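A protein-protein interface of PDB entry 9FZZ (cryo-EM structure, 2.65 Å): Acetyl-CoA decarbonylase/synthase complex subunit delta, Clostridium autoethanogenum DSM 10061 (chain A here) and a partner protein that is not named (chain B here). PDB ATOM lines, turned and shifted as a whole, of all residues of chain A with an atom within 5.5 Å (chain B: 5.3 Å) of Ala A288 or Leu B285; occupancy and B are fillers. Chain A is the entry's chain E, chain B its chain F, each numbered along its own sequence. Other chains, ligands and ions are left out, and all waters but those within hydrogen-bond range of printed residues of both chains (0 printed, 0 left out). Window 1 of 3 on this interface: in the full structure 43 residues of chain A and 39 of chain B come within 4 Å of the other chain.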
ATOM      1  N   PRO A  34       8.496 -19.034  -0.176  1.00  0.00           N
ATOM      2  CA  PRO A  34       9.388 -19.165  -1.339  1.00  0.00           C
ATOM      3  C   PRO A  34      10.502 -20.169  -1.098  1.00  0.00           C
ATOM      4  O   PRO A  34      11.185 -20.146  -0.069  1.00  0.00           O
ATOM      5  CB  PRO A  34       9.939 -17.746  -1.526  1.00  0.00           C
ATOM      6  CG  PRO A  34       8.910 -16.852  -0.894  1.00  0.00           C
ATOM      7  CD  PRO A  34       8.363 -17.635   0.270  1.00  0.00           C
ATOM      8  N   PHE A  35      10.723 -21.026  -2.098  1.00  0.00           N
ATOM      9  CA  PHE A  35      11.758 -22.054  -2.091  1.00  0.00           C
ATOM     10  C   PHE A  35      11.556 -23.093  -0.992  1.00  0.00           C
ATOM     11  O   PHE A  35      12.494 -23.806  -0.632  1.00  0.00           O
ATOM     12  CB  PHE A  35      13.154 -21.430  -1.969  1.00  0.00           C
ATOM     13  CG  PHE A  35      13.412 -20.319  -2.951  1.00  0.00           C
ATOM     14  CD1 PHE A  35      13.478 -20.586  -4.320  1.00  0.00           C
ATOM     15  CD2 PHE A  35      13.586 -19.008  -2.509  1.00  0.00           C
ATOM     16  CE1 PHE A  35      13.710 -19.558  -5.246  1.00  0.00           C
ATOM     17  CE2 PHE A  35      13.820 -17.965  -3.415  1.00  0.00           C
ATOM     18  CZ  PHE A  35      13.881 -18.241  -4.791  1.00  0.00           C
ATOM     19  N   ASP A 226       6.986 -10.240   3.785  1.00  0.00           N
ATOM     20  CA  ASP A 226       6.684 -11.314   4.726  1.00  0.00           C
ATOM     21  C   ASP A 226       5.236 -11.252   5.194  1.00  0.00           C
ATOM     22  O   ASP A 226       4.533 -12.266   5.219  1.00  0.00           O
ATOM     23  CB  ASP A 226       7.613 -11.240   5.934  1.00  0.00           C
ATOM     24  CG  ASP A 226       9.042 -11.603   5.607  1.00  0.00           C
ATOM     25  OD1 ASP A 226       9.247 -12.409   4.676  1.00  0.00           O
ATOM     26  OD2 ASP A 226       9.956 -11.091   6.278  1.00  0.00           O
ATOM     27  N   ALA A 283      17.847  -8.515  -5.323  1.00  0.00           N
ATOM     28  CA  ALA A 283      16.970  -9.506  -5.939  1.00  0.00           C
ATOM     29  C   ALA A 283      16.852 -10.761  -5.089  1.00  0.00           C
ATOM     30  O   ALA A 283      15.754 -11.299  -4.928  1.00  0.00           O
ATOM     31  CB  ALA A 283      17.471  -9.857  -7.339  1.00  0.00           C
ATOM     32  N   SER A 284      17.963 -11.239  -4.529  1.00  0.00           N
ATOM     33  CA  SER A 284      17.911 -12.430  -3.687  1.00  0.00           C
ATOM     34  C   SER A 284      17.056 -12.196  -2.455  1.00  0.00           C
ATOM     35  O   SER A 284      16.259 -13.057  -2.070  1.00  0.00           O
ATOM     36  CB  SER A 284      19.322 -12.841  -3.264  1.00  0.00           C
ATOM     37  OG  SER A 284      20.138 -13.071  -4.401  1.00  0.00           O
ATOM     38  N   GLY A 285      17.198 -11.035  -1.826  1.00  0.00           N
ATOM     39  CA  GLY A 285      16.379 -10.752  -0.659  1.00  0.00           C
ATOM     40  C   GLY A 285      14.895 -10.713  -0.979  1.00  0.00           C
ATOM     41  O   GLY A 285      14.081 -11.331  -0.288  1.00  0.00           O
ATOM     42  N   VAL A 286      14.524 -10.006  -2.049  1.00  0.00           N
ATOM     43  CA  VAL A 286      13.101  -9.896  -2.373  1.00  0.00           C
ATOM     44  C   VAL A 286      12.548 -11.244  -2.829  1.00  0.00           C
ATOM     45  O   VAL A 286      11.397 -11.584  -2.541  1.00  0.00           O
ATOM     46  CB  VAL A 286      12.846  -8.790  -3.413  1.00  0.00           C
ATOM     47  CG1 VAL A 286      13.322  -7.447  -2.878  1.00  0.00           C
ATOM     48  CG2 VAL A 286      13.512  -9.107  -4.738  1.00  0.00           C
ATOM     49  N   LEU A 287      13.353 -12.035  -3.541  1.00  0.00           N
ATOM     50  CA  LEU A 287      12.908 -13.364  -3.950  1.00  0.00           C
ATOM     51  C   LEU A 287      12.696 -14.267  -2.746  1.00  0.00           C
ATOM     52  O   LEU A 287      11.721 -15.021  -2.693  1.00  0.00           O
ATOM     53  CB  LEU A 287      13.920 -13.994  -4.909  1.00  0.00           C
ATOM     54  CG  LEU A 287      13.919 -13.449  -6.341  1.00  0.00           C
ATOM     55  CD1 LEU A 287      15.119 -13.986  -7.091  1.00  0.00           C
ATOM     56  CD2 LEU A 287      12.632 -13.825  -7.063  1.00  0.00           C
ATOM     57  N   ALA A 288      13.598 -14.206  -1.769  1.00  0.00           N
ATOM     58  CA  ALA A 288      13.422 -15.017  -0.574  1.00  0.00           C
ATOM     59  C   ALA A 288      12.239 -14.550   0.260  1.00  0.00           C
ATOM     60  O   ALA A 288      11.625 -15.359   0.961  1.00  0.00           O
ATOM     61  CB  ALA A 288      14.700 -14.998   0.266  1.00  0.00           C
ATOM     62  N   SER A 289      11.911 -13.257   0.214  1.00  0.00           N
ATOM     63  CA  SER A 289      10.816 -12.737   1.026  1.00  0.00           C
ATOM     64  C   SER A 289       9.439 -12.936   0.410  1.00  0.00           C
ATOM     65  O   SER A 289       8.440 -12.810   1.126  1.00  0.00           O
ATOM     66  CB  SER A 289      11.006 -11.244   1.290  1.00  0.00           C
ATOM     67  OG  SER A 289      12.122 -11.038   2.132  1.00  0.00           O
ATOM     68  N   GLY A 290       9.349 -13.253  -0.879  1.00  0.00           N
ATOM     69  CA  GLY A 290       8.052 -13.581  -1.437  1.00  0.00           C
ATOM     70  C   GLY A 290       7.681 -12.945  -2.764  1.00  0.00           C
ATOM     71  O   GLY A 290       6.524 -13.056  -3.176  1.00  0.00           O
ATOM     72  N   PHE A 308      20.787 -18.855  -9.256  1.00  0.00           N
ATOM     73  CA  PHE A 308      20.361 -18.925  -7.856  1.00  0.00           C
ATOM     74  C   PHE A 308      18.985 -19.566  -7.724  1.00  0.00           C
ATOM     75  O   PHE A 308      18.770 -20.450  -6.880  1.00  0.00           O
ATOM     76  CB  PHE A 308      20.397 -17.502  -7.288  1.00  0.00           C
ATOM     77  CG  PHE A 308      19.766 -17.341  -5.932  1.00  0.00           C
ATOM     78  CD1 PHE A 308      20.460 -17.697  -4.776  1.00  0.00           C
ATOM     79  CD2 PHE A 308      18.499 -16.780  -5.810  1.00  0.00           C
ATOM     80  CE1 PHE A 308      19.882 -17.532  -3.511  1.00  0.00           C
ATOM     81  CE2 PHE A 308      17.905 -16.605  -4.557  1.00  0.00           C
ATOM     82  CZ  PHE A 308      18.600 -16.982  -3.402  1.00  0.00           C
ATOM     83  N   LEU A 312      18.139 -23.221  -5.967  1.00  0.00           N
ATOM     84  CA  LEU A 312      17.225 -23.350  -4.836  1.00  0.00           C
ATOM     85  C   LEU A 312      16.038 -24.249  -5.164  1.00  0.00           C
ATOM     86  O   LEU A 312      15.644 -25.082  -4.343  1.00  0.00           O
ATOM     87  CB  LEU A 312      16.751 -21.971  -4.373  1.00  0.00           C
ATOM     88  CG  LEU A 312      17.714 -21.225  -3.436  1.00  0.00           C
ATOM     89  CD1 LEU A 312      17.040 -19.990  -2.888  1.00  0.00           C
ATOM     90  CD2 LEU A 312      18.193 -22.098  -2.279  1.00  0.00           C
ATOM     91  N   PHE B 242      19.921 -25.344   2.391  1.00  0.00           N
ATOM     92  CA  PHE B 242      18.841 -24.412   2.709  1.00  0.00           C
ATOM     93  C   PHE B 242      17.714 -25.114   3.454  1.00  0.00           C
ATOM     94  O   PHE B 242      17.190 -24.589   4.447  1.00  0.00           O
ATOM     95  CB  PHE B 242      18.325 -23.759   1.426  1.00  0.00           C
ATOM     96  CG  PHE B 242      17.131 -22.875   1.633  1.00  0.00           C
ATOM     97  CD1 PHE B 242      17.274 -21.618   2.217  1.00  0.00           C
ATOM     98  CD2 PHE B 242      15.864 -23.300   1.248  1.00  0.00           C
ATOM     99  CE1 PHE B 242      16.166 -20.790   2.423  1.00  0.00           C
ATOM    100  CE2 PHE B 242      14.743 -22.488   1.443  1.00  0.00           C
ATOM    101  CZ  PHE B 242      14.895 -21.227   2.034  1.00  0.00           C
ATOM    102  N   VAL B 280      27.343 -13.803  -2.729  1.00  0.00           N
ATOM    103  CA  VAL B 280      26.495 -12.679  -2.332  1.00  0.00           C
ATOM    104  C   VAL B 280      25.032 -13.103  -2.289  1.00  0.00           C
ATOM    105  O   VAL B 280      24.298 -12.768  -1.352  1.00  0.00           O
ATOM    106  CB  VAL B 280      26.719 -11.486  -3.273  1.00  0.00           C
ATOM    107  CG1 VAL B 280      25.771 -10.347  -2.931  1.00  0.00           C
ATOM    108  CG2 VAL B 280      28.157 -11.007  -3.176  1.00  0.00           C
ATOM    109  N   ALA B 281      24.582 -13.840  -3.302  1.00  0.00           N
ATOM    110  CA  ALA B 281      23.188 -14.279  -3.331  1.00  0.00           C
ATOM    111  C   ALA B 281      22.869 -15.172  -2.139  1.00  0.00           C
ATOM    112  O   ALA B 281      21.859 -14.980  -1.450  1.00  0.00           O
ATOM    113  CB  ALA B 281      22.891 -15.003  -4.644  1.00  0.00           C
ATOM    114  N   LEU B 282      23.726 -16.154  -1.870  1.00  0.00           N
ATOM    115  CA  LEU B 282      23.476 -17.062  -0.757  1.00  0.00           C
ATOM    116  C   LEU B 282      23.617 -16.366   0.588  1.00  0.00           C
ATOM    117  O   LEU B 282      22.891 -16.694   1.528  1.00  0.00           O
ATOM    118  CB  LEU B 282      24.404 -18.273  -0.837  1.00  0.00           C
ATOM    119  CG  LEU B 282      24.086 -19.278  -1.956  1.00  0.00           C
ATOM    120  CD1 LEU B 282      24.835 -20.569  -1.686  1.00  0.00           C
ATOM    121  CD2 LEU B 282      22.592 -19.566  -2.098  1.00  0.00           C
ATOM    122  N   SER B 283      24.542 -15.414   0.709  1.00  0.00           N
ATOM    123  CA  SER B 283      24.671 -14.669   1.955  1.00  0.00           C
ATOM    124  C   SER B 283      23.432 -13.830   2.220  1.00  0.00           C
ATOM    125  O   SER B 283      22.957 -13.762   3.354  1.00  0.00           O
ATOM    126  CB  SER B 283      25.911 -13.772   1.912  1.00  0.00           C
ATOM    127  OG  SER B 283      27.052 -14.501   1.479  1.00  0.00           O
ATOM    128  N   THR B 284      22.889 -13.192   1.183  1.00  0.00           N
ATOM    129  CA  THR B 284      21.641 -12.455   1.354  1.00  0.00           C
ATOM    130  C   THR B 284      20.496 -13.391   1.706  1.00  0.00           C
ATOM    131  O   THR B 284      19.615 -13.038   2.493  1.00  0.00           O
ATOM    132  CB  THR B 284      21.304 -11.670   0.091  1.00  0.00           C
ATOM    133  OG1 THR B 284      22.452 -10.939  -0.354  1.00  0.00           O
ATOM    134  CG2 THR B 284      20.187 -10.699   0.381  1.00  0.00           C
ATOM    135  N   LEU B 285      20.485 -14.588   1.120  1.00  0.00           N
ATOM    136  CA  LEU B 285      19.456 -15.564   1.460  1.00  0.00           C
ATOM    137  C   LEU B 285      19.533 -15.961   2.929  1.00  0.00           C
ATOM    138  O   LEU B 285      18.520 -15.979   3.633  1.00  0.00           O
ATOM    139  CB  LEU B 285      19.595 -16.796   0.563  1.00  0.00           C
ATOM    140  CG  LEU B 285      18.718 -17.997   0.941  1.00  0.00           C
ATOM    141  CD1 LEU B 285      17.249 -17.720   0.643  1.00  0.00           C
ATOM    142  CD2 LEU B 285      19.198 -19.234   0.210  1.00  0.00           C
ATOM    143  N   PHE B 286      20.730 -16.302   3.406  1.00  0.00           N
ATOM    144  CA  PHE B 286      20.881 -16.816   4.760  1.00  0.00           C
ATOM    145  C   PHE B 286      20.926 -15.722   5.817  1.00  0.00           C
ATOM    146  O   PHE B 286      20.843 -16.039   7.005  1.00  0.00           O
ATOM    147  CB  PHE B 286      22.135 -17.686   4.859  1.00  0.00           C
ATOM    148  CG  PHE B 286      22.005 -19.012   4.166  1.00  0.00           C
ATOM    149  CD1 PHE B 286      21.091 -19.959   4.625  1.00  0.00           C
ATOM    150  CD2 PHE B 286      22.781 -19.312   3.052  1.00  0.00           C
ATOM    151  CE1 PHE B 286      20.951 -21.197   3.981  1.00  0.00           C
ATOM    152  CE2 PHE B 286      22.659 -20.542   2.395  1.00  0.00           C
ATOM    153  CZ  PHE B 286      21.740 -21.489   2.862  1.00  0.00           C
ATOM    154  N   THR B 287      21.083 -14.457   5.423  1.00  0.00           N
ATOM    155  CA  THR B 287      20.852 -13.378   6.375  1.00  0.00           C
ATOM    156  C   THR B 287      19.398 -13.350   6.810  1.00  0.00           C
ATOM    157  O   THR B 287      19.095 -13.100   7.981  1.00  0.00           O
ATOM    158  CB  THR B 287      21.233 -12.035   5.748  1.00  0.00           C
ATOM    159  OG1 THR B 287      22.611 -12.038   5.358  1.00  0.00           O
ATOM    160  CG2 THR B 287      20.996 -10.902   6.728  1.00  0.00           C
ATOM    161  N   LEU B 288      18.484 -13.617   5.881  1.00  0.00           N
ATOM    162  CA  LEU B 288      17.068 -13.674   6.205  1.00  0.00           C
ATOM    163  C   LEU B 288      16.591 -15.066   6.575  1.00  0.00           C
ATOM    164  O   LEU B 288      15.497 -15.207   7.129  1.00  0.00           O
ATOM    165  CB  LEU B 288      16.252 -13.181   5.003  1.00  0.00           C
ATOM    166  CG  LEU B 288      16.429 -11.695   4.674  1.00  0.00           C
ATOM    167  CD1 LEU B 288      15.948 -11.387   3.268  1.00  0.00           C
ATOM    168  CD2 LEU B 288      15.661 -10.879   5.699  1.00  0.00           C
ATOM    169  N   LYS B 289      17.388 -16.089   6.273  1.00  0.00           N
ATOM    170  CA  LYS B 289      16.971 -17.472   6.452  1.00  0.00           C
ATOM    171  C   LYS B 289      17.772 -18.235   7.502  1.00  0.00           C
ATOM    172  O   LYS B 289      18.225 -19.356   7.251  1.00  0.00           O
ATOM    173  CB  LYS B 289      16.956 -18.189   5.100  1.00  0.00           C
ATOM    174  CG  LYS B 289      15.812 -17.653   4.208  1.00  0.00           C
ATOM    175  CD  LYS B 289      14.444 -18.201   4.654  1.00  0.00           C
ATOM    176  CE  LYS B 289      13.403 -17.087   4.814  1.00  0.00           C
ATOM    177  NZ  LYS B 289      12.109 -17.640   5.348  1.00  0.00           N
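Among the printed residues, merely in contact across the chains: Phe A35 with Phe B242, Ser A284 with Ala B281, Gly A285 with Thr B284, Ala A288 with Leu B285, Phe A308 with Ala B281, Phe A308 with Leu B282 and Leu A312 with Leu B285.
The backbone carbonyl oxygen (O) of Gly A285 lies within hydrogen-bond range of the side-chain hydroxyl (OG) of Ser A289 (3.1 Å).
O of Val B280 is in hydrogen-bond range of OG1 of Thr B284 (2.8 Å).
Of the printed residues of chain B, Phe A35 touches Phe B242 (3.3 Å).
Of the printed residues of chain B, Ser A284 touches Ala B281.
Of chain B, only Leu B285 comes within 4 Å of Ala A288.
Printed residues of chain B within 4 Å of Phe A308: Ala B281 and Leu B282.
Printed residues of chain A within 4 Å of Phe B242: Phe A35 (3.3 Å).
Of the printed residues of chain A, Leu B285 touches Ala A288 (3.7 Å) and Leu A312 (3.9 Å).
The nearest residue of chain B that does not touch Ala A288 is Lys B289 (4.6 Å).
The nearest printed residue of chain B that does not touch Ser A284 is Thr B284 (4.1 Å).
Of the 11 printed residues of chain B, 5 touch a printed residue of chain A.
Printed residues of chain B that touch a printed residue of chain A: Phe B242, Ala B281, Leu B282, Thr B284 and Leu B285.
Hydrophobic or aromatic side chains of chain B within 4 Å of the printed part of chain A: Phe B242, Ala B281, Leu B282 and Leu B285.
Hydrophobic or aromatic side chains of chain A that line the printed part of chain B: Phe A35, Ala A288, Phe A308 and Leu A312.
Among the printed residues, 7 pairs touch across the chains.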
